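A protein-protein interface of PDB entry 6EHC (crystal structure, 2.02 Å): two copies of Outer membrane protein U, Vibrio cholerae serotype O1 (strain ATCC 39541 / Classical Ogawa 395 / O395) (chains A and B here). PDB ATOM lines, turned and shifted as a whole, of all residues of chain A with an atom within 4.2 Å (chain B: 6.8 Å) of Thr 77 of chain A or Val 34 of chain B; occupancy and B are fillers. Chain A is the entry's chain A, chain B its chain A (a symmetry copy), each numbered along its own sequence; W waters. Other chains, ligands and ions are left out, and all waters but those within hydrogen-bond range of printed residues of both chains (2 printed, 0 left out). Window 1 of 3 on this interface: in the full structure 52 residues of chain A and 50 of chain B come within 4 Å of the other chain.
The backbone carbonyl oxygen (O) of Thr 77 of chain A sits at hydrogen-bond distance from the backbone NH (N) of Lys 92 of chain A (3.1 Å). The backbone carbonyl oxygen (O) of Val 34 of chain B is in hydrogen-bond range of the backbone NH (N) of Phe 58 of chain B. OD1 of Asp 30 of chain B is in hydrogen-bond range of OG of Ser 32 of chain B, at 2.6 Å. The backbone carbonyl oxygen of Tyr 78 of chain A sits at hydrogen-bond distance from the backbone NH of Phe 53 of chain A (3.0 Å).
Among the printed residues, pairs that only touch across the chains: Phe 53 of chain A with Ala 17 of chain B, Tyr 54 of chain A with Val 34 of chain B, Tyr 54 of chain A with Phe 58 of chain B, Thr 77 of chain A with Val 34 of chain B, Thr 77 of chain A with Thr 60 of chain B, Tyr 78 of chain A with Ala 17 of chain B, Gly 91 of chain A with Asp 30 of chain B and Gly 91 of chain A with Ser 32 of chain B.
Of chain B, only Val 34 (3.9 Å) and Thr 60 (3.7 Å) come within 4 Å of Thr 77 of chain A. Val 34 of chain B touches two residues of chain A. Printed residues of chain A within 4 Å of Phe 58 of chain B: Tyr 54 (3.3 Å). Of the printed residues of chain A, Asp 30 of chain B touches Gly 91 (3.8 Å). Glu 18 of chain B touches none of the printed residues of chain A. Arg 16 of chain B touches none of the printed residues of chain A. The nearest residue of chain B that does not touch Thr 77 of chain A is Phe 58 of chain B (4.3 Å). The nearest printed residue of chain B that does not touch Tyr 54 of chain A is Leu 36 of chain B (4.01 Å).
Hydrophobic or aromatic side chains of chain A that line the printed part of chain B: Tyr 54. Of the 17 printed residues of chain B, 6 touch a printed residue of chain A. Hydrophobic or aromatic side chains of chain B that line the printed part of chain A: Ala 17, Val 34 and Phe 58. Along chain B the printed residues that touch a printed residue of chain A span positions 17 to 60. Among the printed residues, no Asp or Glu carboxylate lies within 4 Å of a Lys or Arg side-chain nitrogen of the other chain.
No position is printed for both chains. Of the 8 pairs that touch across the chains among the printed residues, none has its exchanged pair printed and touching as well.
Water W2 lies within hydrogen-bond range of the side-chain hydroxyl of Thr 60 of chain B, the side-chain carboxylate of Asp 30 of chain B, the side-chain hydroxyl of Thr 77 of chain A and the backbone NH of Lys 92 of chain A. Water W1 lies within hydrogen-bond range of O of Ser 32 of chain B (2.9 Å), OG1 of Thr 77 of chain A (2.9 Å) and N of Thr 60 of chain B (3.0 Å).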
ATOM      1  N   PHE A  53      27.437  -4.461  13.655  1.00  0.00           N
ATOM      2  CA  PHE A  53      26.312  -3.479  13.681  1.00  0.00           C
ATOM      3  C   PHE A  53      24.964  -4.104  14.013  1.00  0.00           C
ATOM      4  O   PHE A  53      24.573  -5.113  13.406  1.00  0.00           O
ATOM      5  CB  PHE A  53      26.184  -2.726  12.322  1.00  0.00           C
ATOM      6  CG  PHE A  53      25.209  -1.549  12.338  1.00  0.00           C
ATOM      7  CD1 PHE A  53      25.490  -0.398  13.065  1.00  0.00           C
ATOM      8  CD2 PHE A  53      24.004  -1.591  11.624  1.00  0.00           C
ATOM      9  CE1 PHE A  53      24.591   0.699  13.056  1.00  0.00           C
ATOM     10  CE2 PHE A  53      23.103  -0.525  11.646  1.00  0.00           C
ATOM     11  CZ  PHE A  53      23.409   0.629  12.366  1.00  0.00           C
ATOM     12  N   TYR A  54      24.215  -3.439  14.907  1.00  0.00           N
ATOM     13  CA  TYR A  54      22.806  -3.770  15.170  1.00  0.00           C
ATOM     14  C   TYR A  54      21.916  -2.497  15.091  1.00  0.00           C
ATOM     15  O   TYR A  54      22.305  -1.436  15.569  1.00  0.00           O
ATOM     16  CB  TYR A  54      22.644  -4.466  16.572  1.00  0.00           C
ATOM     17  CG  TYR A  54      21.136  -4.582  16.982  1.00  0.00           C
ATOM     18  CD1 TYR A  54      20.301  -5.528  16.370  1.00  0.00           C
ATOM     19  CD2 TYR A  54      20.536  -3.673  17.852  1.00  0.00           C
ATOM     20  CE1 TYR A  54      18.961  -5.603  16.658  1.00  0.00           C
ATOM     21  CE2 TYR A  54      19.173  -3.731  18.137  1.00  0.00           C
ATOM     22  CZ  TYR A  54      18.385  -4.707  17.552  1.00  0.00           C
ATOM     23  OH  TYR A  54      17.019  -4.801  17.795  1.00  0.00           O
ATOM     24  N   TYR A  76      18.767  -4.402  11.218  1.00  0.00           N
ATOM     25  CA  TYR A  76      20.136  -4.718  10.691  1.00  0.00           C
ATOM     26  C   TYR A  76      20.764  -5.653  11.681  1.00  0.00           C
ATOM     27  O   TYR A  76      20.657  -5.374  12.879  1.00  0.00           O
ATOM     28  CB  TYR A  76      21.028  -3.468  10.625  1.00  0.00           C
ATOM     29  CG  TYR A  76      20.745  -2.504   9.503  1.00  0.00           C
ATOM     30  CD1 TYR A  76      19.804  -1.460   9.669  1.00  0.00           C
ATOM     31  CD2 TYR A  76      21.484  -2.531   8.312  1.00  0.00           C
ATOM     32  CE1 TYR A  76      19.549  -0.532   8.646  1.00  0.00           C
ATOM     33  CE2 TYR A  76      21.243  -1.597   7.298  1.00  0.00           C
ATOM     34  CZ  TYR A  76      20.264  -0.598   7.469  1.00  0.00           C
ATOM     35  OH  TYR A  76      19.984   0.319   6.455  1.00  0.00           O
ATOM     36  N   THR A  77      21.364  -6.780  11.222  1.00  0.00           N
ATOM     37  CA  THR A  77      22.203  -7.664  12.090  1.00  0.00           C
ATOM     38  C   THR A  77      23.371  -8.235  11.243  1.00  0.00           C
ATOM     39  O   THR A  77      23.160  -9.156  10.450  1.00  0.00           O
ATOM     40  CB  THR A  77      21.422  -8.866  12.702  1.00  0.00           C
ATOM     41  OG1 THR A  77      20.822  -9.659  11.675  1.00  0.00           O
ATOM     42  CG2 THR A  77      20.308  -8.432  13.669  1.00  0.00           C
ATOM     43  N   TYR A  78      24.566  -7.671  11.375  1.00  0.00           N
ATOM     44  CA  TYR A  78      25.665  -8.000  10.499  1.00  0.00           C
ATOM     45  C   TYR A  78      27.049  -7.789  11.127  1.00  0.00           C
ATOM     46  O   TYR A  78      27.210  -7.046  12.107  1.00  0.00           O
ATOM     47  CB  TYR A  78      25.548  -7.310   9.107  1.00  0.00           C
ATOM     48  CG  TYR A  78      25.906  -5.855   9.031  1.00  0.00           C
ATOM     49  CD1 TYR A  78      27.236  -5.446   9.066  1.00  0.00           C
ATOM     50  CD2 TYR A  78      24.891  -4.860   8.875  1.00  0.00           C
ATOM     51  CE1 TYR A  78      27.580  -4.108   8.974  1.00  0.00           C
ATOM     52  CE2 TYR A  78      25.214  -3.504   8.758  1.00  0.00           C
ATOM     53  CZ  TYR A  78      26.553  -3.135   8.787  1.00  0.00           C
ATOM     54  OH  TYR A  78      26.885  -1.815   8.713  1.00  0.00           O
ATOM     55  N   GLY A  91      24.794 -11.101   6.802  1.00  0.00           N
ATOM     56  CA  GLY A  91      23.681 -10.896   7.759  1.00  0.00           C
ATOM     57  C   GLY A  91      22.813  -9.753   7.195  1.00  0.00           C
ATOM     58  O   GLY A  91      23.219  -9.144   6.228  1.00  0.00           O
ATOM     59  N   LYS A  92      21.648  -9.440   7.784  1.00  0.00           N
ATOM     60  CA  LYS A  92      20.714  -8.436   7.209  1.00  0.00           C
ATOM     61  C   LYS A  92      21.369  -7.088   7.079  1.00  0.00           C
ATOM     62  O   LYS A  92      21.730  -6.457   8.105  1.00  0.00           O
ATOM     63  CB  LYS A  92      19.381  -8.328   7.984  1.00  0.00           C
ATOM     64  CG  LYS A  92      18.311  -7.476   7.316  1.00  0.00           C
ATOM     65  CD  LYS A  92      16.887  -7.798   7.733  1.00  0.00           C
ATOM     66  CE  LYS A  92      15.878  -6.942   6.939  1.00  0.00           C
ATOM     67  NZ  LYS A  92      14.449  -7.395   7.014  1.00  0.00           N
ATOM     68  N   GLY B  15      28.422  -7.619  24.365  1.00  0.00           N
ATOM     69  CA  GLY B  15      27.660  -8.477  23.497  1.00  0.00           C
ATOM     70  C   GLY B  15      28.455  -8.813  22.215  1.00  0.00           C
ATOM     71  O   GLY B  15      29.705  -8.775  22.208  1.00  0.00           O
ATOM     72  N   ARG B  16      27.713  -9.129  21.146  1.00  0.00           N
ATOM     73  CA  ARG B  16      28.340  -9.491  19.853  1.00  0.00           C
ATOM     74  C   ARG B  16      27.471  -9.205  18.636  1.00  0.00           C
ATOM     75  O   ARG B  16      26.224  -9.118  18.733  1.00  0.00           O
ATOM     76  CB  ARG B  16      28.781 -10.990  19.875  1.00  0.00           C
ATOM     77  CG  ARG B  16      27.614 -11.943  19.700  1.00  0.00           C
ATOM     78  CD  ARG B  16      28.022 -13.381  19.752  1.00  0.00           C
ATOM     79  NE  ARG B  16      28.429 -13.794  21.093  1.00  0.00           N
ATOM     80  CZ  ARG B  16      28.806 -15.027  21.404  1.00  0.00           C
ATOM     81  NH1 ARG B  16      28.864 -15.979  20.473  1.00  0.00           N
ATOM     82  NH2 ARG B  16      29.199 -15.304  22.641  1.00  0.00           N
ATOM     83  N   ALA B  17      28.142  -9.066  17.482  1.00  0.00           N
ATOM     84  CA  ALA B  17      27.508  -9.175  16.171  1.00  0.00           C
ATOM     85  C   ALA B  17      28.211 -10.303  15.419  1.00  0.00           C
ATOM     86  O   ALA B  17      29.432 -10.206  15.126  1.00  0.00           O
ATOM     87  CB  ALA B  17      27.617  -7.870  15.420  1.00  0.00           C
ATOM     88  N   GLU B  18      27.452 -11.366  15.114  1.00  0.00           N
ATOM     89  CA  GLU B  18      28.024 -12.648  14.683  1.00  0.00           C
ATOM     90  C   GLU B  18      27.330 -13.185  13.459  1.00  0.00           C
ATOM     91  O   GLU B  18      26.211 -13.674  13.548  1.00  0.00           O
ATOM     92  CB  GLU B  18      28.040 -13.705  15.858  1.00  0.00           C
ATOM     93  CG  GLU B  18      28.805 -14.994  15.439  1.00  0.00           C
ATOM     94  CD  GLU B  18      28.988 -16.072  16.519  1.00  0.00           C
ATOM     95  OE1 GLU B  18      28.243 -16.012  17.534  1.00  0.00           O
ATOM     96  OE2 GLU B  18      29.876 -16.986  16.350  1.00  0.00           O
ATOM     97  N   ALA B  19      27.966 -12.971  12.310  1.00  0.00           N
ATOM     98  CA  ALA B  19      27.532 -13.454  11.026  1.00  0.00           C
ATOM     99  C   ALA B  19      27.850 -14.938  10.910  1.00  0.00           C
ATOM    100  O   ALA B  19      28.992 -15.320  11.153  1.00  0.00           O
ATOM    101  CB  ALA B  19      28.275 -12.711   9.940  1.00  0.00           C
ATOM    102  N   ASP B  30      20.877 -18.664   7.122  1.00  0.00           N
ATOM    103  CA  ASP B  30      21.465 -17.547   7.868  1.00  0.00           C
ATOM    104  C   ASP B  30      21.195 -17.799   9.357  1.00  0.00           C
ATOM    105  O   ASP B  30      20.032 -17.693   9.808  1.00  0.00           O
ATOM    106  CB  ASP B  30      20.868 -16.168   7.409  1.00  0.00           C
ATOM    107  CG  ASP B  30      21.601 -14.973   7.991  1.00  0.00           C
ATOM    108  OD1 ASP B  30      22.371 -15.147   8.980  1.00  0.00           O
ATOM    109  OD2 ASP B  30      21.345 -13.834   7.508  1.00  0.00           O
ATOM    110  N   SER B  32      22.857 -16.048  11.728  1.00  0.00           N
ATOM    111  CA  SER B  32      23.495 -14.860  12.319  1.00  0.00           C
ATOM    112  C   SER B  32      22.698 -14.363  13.551  1.00  0.00           C
ATOM    113  O   SER B  32      21.497 -14.617  13.693  1.00  0.00           O
ATOM    114  CB  SER B  32      23.604 -13.712  11.285  1.00  0.00           C
ATOM    115  OG  SER B  32      24.403 -14.032  10.106  1.00  0.00           O
ATOM    116  N   ARG B  33      23.382 -13.688  14.466  1.00  0.00           N
ATOM    117  CA  ARG B  33      22.731 -13.135  15.633  1.00  0.00           C
ATOM    118  C   ARG B  33      23.536 -12.004  16.252  1.00  0.00           C
ATOM    119  O   ARG B  33      24.766 -11.950  16.091  1.00  0.00           O
ATOM    120  CB  ARG B  33      22.472 -14.245  16.697  1.00  0.00           C
ATOM    121  CG  ARG B  33      23.654 -14.698  17.561  1.00  0.00           C
ATOM    122  CD  ARG B  33      24.269 -15.977  17.004  1.00  0.00           C
ATOM    123  NE  ARG B  33      25.412 -16.559  17.740  1.00  0.00           N
ATOM    124  CZ  ARG B  33      25.382 -17.580  18.589  1.00  0.00           C
ATOM    125  NH1 ARG B  33      24.265 -18.159  18.939  1.00  0.00           N
ATOM    126  NH2 ARG B  33      26.517 -18.038  19.118  1.00  0.00           N
ATOM    127  N   VAL B  34      22.815 -11.135  16.954  1.00  0.00           N
ATOM    128  CA  VAL B  34      23.341 -10.106  17.786  1.00  0.00           C
ATOM    129  C   VAL B  34      22.961 -10.422  19.236  1.00  0.00           C
ATOM    130  O   VAL B  34      21.842 -10.866  19.514  1.00  0.00           O
ATOM    131  CB  VAL B  34      22.792  -8.702  17.395  1.00  0.00           C
ATOM    132  CG1 VAL B  34      23.075  -7.616  18.476  1.00  0.00           C
ATOM    133  CG2 VAL B  34      23.371  -8.269  16.068  1.00  0.00           C
ATOM    134  N   ARG B  35      23.905 -10.169  20.141  1.00  0.00           N
ATOM    135  CA  ARG B  35      23.646 -10.126  21.594  1.00  0.00           C
ATOM    136  C   ARG B  35      24.052  -8.745  22.158  1.00  0.00           C
ATOM    137  O   ARG B  35      25.153  -8.197  21.802  1.00  0.00           O
ATOM    138  CB  ARG B  35      24.448 -11.216  22.311  1.00  0.00           C
ATOM    139  CG  ARG B  35      23.803 -12.587  22.228  1.00  0.00           C
ATOM    140  CD  ARG B  35      24.646 -13.693  22.813  1.00  0.00           C
ATOM    141  NE  ARG B  35      24.126 -15.002  22.412  1.00  0.00           N
ATOM    142  CZ  ARG B  35      24.691 -16.166  22.737  1.00  0.00           C
ATOM    143  NH1 ARG B  35      25.757 -16.178  23.539  1.00  0.00           N
ATOM    144  NH2 ARG B  35      24.152 -17.312  22.336  1.00  0.00           N
ATOM    145  N   LEU B  36      23.194  -8.200  23.031  1.00  0.00           N
ATOM    146  CA  LEU B  36      23.496  -6.942  23.737  1.00  0.00           C
ATOM    147  C   LEU B  36      23.385  -7.193  25.227  1.00  0.00           C
ATOM    148  O   LEU B  36      22.402  -7.809  25.642  1.00  0.00           O
ATOM    149  CB  LEU B  36      22.526  -5.818  23.350  1.00  0.00           C
ATOM    150  CG  LEU B  36      22.473  -5.328  21.882  1.00  0.00           C
ATOM    151  CD1 LEU B  36      21.387  -4.291  21.718  1.00  0.00           C
ATOM    152  CD2 LEU B  36      23.789  -4.751  21.388  1.00  0.00           C
ATOM    153  N   GLY B  56      20.150  -9.782  25.944  1.00  0.00           N
ATOM    154  CA  GLY B  56      19.150 -10.155  24.958  1.00  0.00           C
ATOM    155  C   GLY B  56      19.808 -10.685  23.699  1.00  0.00           C
ATOM    156  O   GLY B  56      20.945 -10.261  23.367  1.00  0.00           O
ATOM    157  N   GLU B  57      19.084 -11.570  22.984  1.00  0.00           N
ATOM    158  CA  GLU B  57      19.522 -12.069  21.651  1.00  0.00           C
ATOM    159  C   GLU B  57      18.505 -11.727  20.574  1.00  0.00           C
ATOM    160  O   GLU B  57      17.315 -11.907  20.778  1.00  0.00           O
ATOM    161  CB  GLU B  57      19.774 -13.612  21.658  1.00  0.00           C
ATOM    162  CG  GLU B  57      20.308 -14.163  20.337  1.00  0.00           C
ATOM    163  CD  GLU B  57      20.799 -15.628  20.431  1.00  0.00           C
ATOM    164  OE1 GLU B  57      20.031 -16.508  20.011  1.00  0.00           O
ATOM    165  OE2 GLU B  57      21.922 -15.885  20.925  1.00  0.00           O
ATOM    166  N   PHE B  58      18.997 -11.295  19.424  1.00  0.00           N
ATOM    167  CA  PHE B  58      18.203 -10.589  18.399  1.00  0.00           C
ATOM    168  C   PHE B  58      18.570 -11.265  17.072  1.00  0.00           C
ATOM    169  O   PHE B  58      19.780 -11.323  16.753  1.00  0.00           O
ATOM    170  CB  PHE B  58      18.626  -9.106  18.332  1.00  0.00           C
ATOM    171  CG  PHE B  58      18.391  -8.298  19.611  1.00  0.00           C
ATOM    172  CD1 PHE B  58      19.300  -8.330  20.662  1.00  0.00           C
ATOM    173  CD2 PHE B  58      17.279  -7.493  19.747  1.00  0.00           C
ATOM    174  CE1 PHE B  58      19.099  -7.582  21.823  1.00  0.00           C
ATOM    175  CE2 PHE B  58      17.074  -6.734  20.921  1.00  0.00           C
ATOM    176  CZ  PHE B  58      17.974  -6.773  21.944  1.00  0.00           C
ATOM    177  N   THR B  59      17.581 -11.824  16.338  1.00  0.00           N
ATOM    178  CA  THR B  59      17.820 -12.469  15.045  1.00  0.00           C
ATOM    179  C   THR B  59      16.853 -12.016  13.957  1.00  0.00           C
ATOM    180  O   THR B  59      15.862 -11.308  14.232  1.00  0.00           O
ATOM    181  CB  THR B  59      17.748 -14.036  15.132  1.00  0.00           C
ATOM    182  OG1 THR B  59      16.406 -14.428  15.437  1.00  0.00           O
ATOM    183  CG2 THR B  59      18.698 -14.568  16.198  1.00  0.00           C
ATOM    184  N   THR B  60      17.104 -12.498  12.732  1.00  0.00           N
ATOM    185  CA  THR B  60      16.204 -12.293  11.542  1.00  0.00           C
ATOM    186  C   THR B  60      15.822 -13.608  10.879  1.00  0.00           C
ATOM    187  O   THR B  60      16.508 -14.582  11.034  1.00  0.00           O
ATOM    188  CB  THR B  60      16.796 -11.308  10.492  1.00  0.00           C
ATOM    189  OG1 THR B  60      17.955 -11.870   9.806  1.00  0.00           O
ATOM    190  CG2 THR B  60      17.133 -10.002  11.186  1.00  0.00           C
ATOM    191  N   PHE B 309      31.491  -6.589  21.122  1.00  0.00           N
ATOM    192  CA  PHE B 309      31.390  -5.198  21.552  1.00  0.00           C
ATOM    193  C   PHE B 309      32.242  -4.867  22.831  1.00  0.00           C
ATOM    194  O   PHE B 309      32.484  -5.640  23.794  1.00  0.00           O
ATOM    195  CB  PHE B 309      29.930  -4.809  21.772  1.00  0.00           C
ATOM    196  CG  PHE B 309      29.068  -4.791  20.536  1.00  0.00           C
ATOM    197  CD1 PHE B 309      29.282  -3.862  19.532  1.00  0.00           C
ATOM    198  CD2 PHE B 309      27.933  -5.617  20.445  1.00  0.00           C
ATOM    199  CE1 PHE B 309      28.436  -3.777  18.426  1.00  0.00           C
ATOM    200  CE2 PHE B 309      27.078  -5.546  19.349  1.00  0.00           C
ATOM    201  CZ  PHE B 309      27.341  -4.620  18.321  1.00  0.00           C
ATOM    202  OXT PHE B 309      32.708  -3.724  22.930  1.00  0.00           O
HETATM  203  O   HOH W   1      20.117 -12.328  12.660  1.00  0.00           O
HETATM  204  O   HOH W   2      20.750 -11.927   9.555  1.00  0.00           O
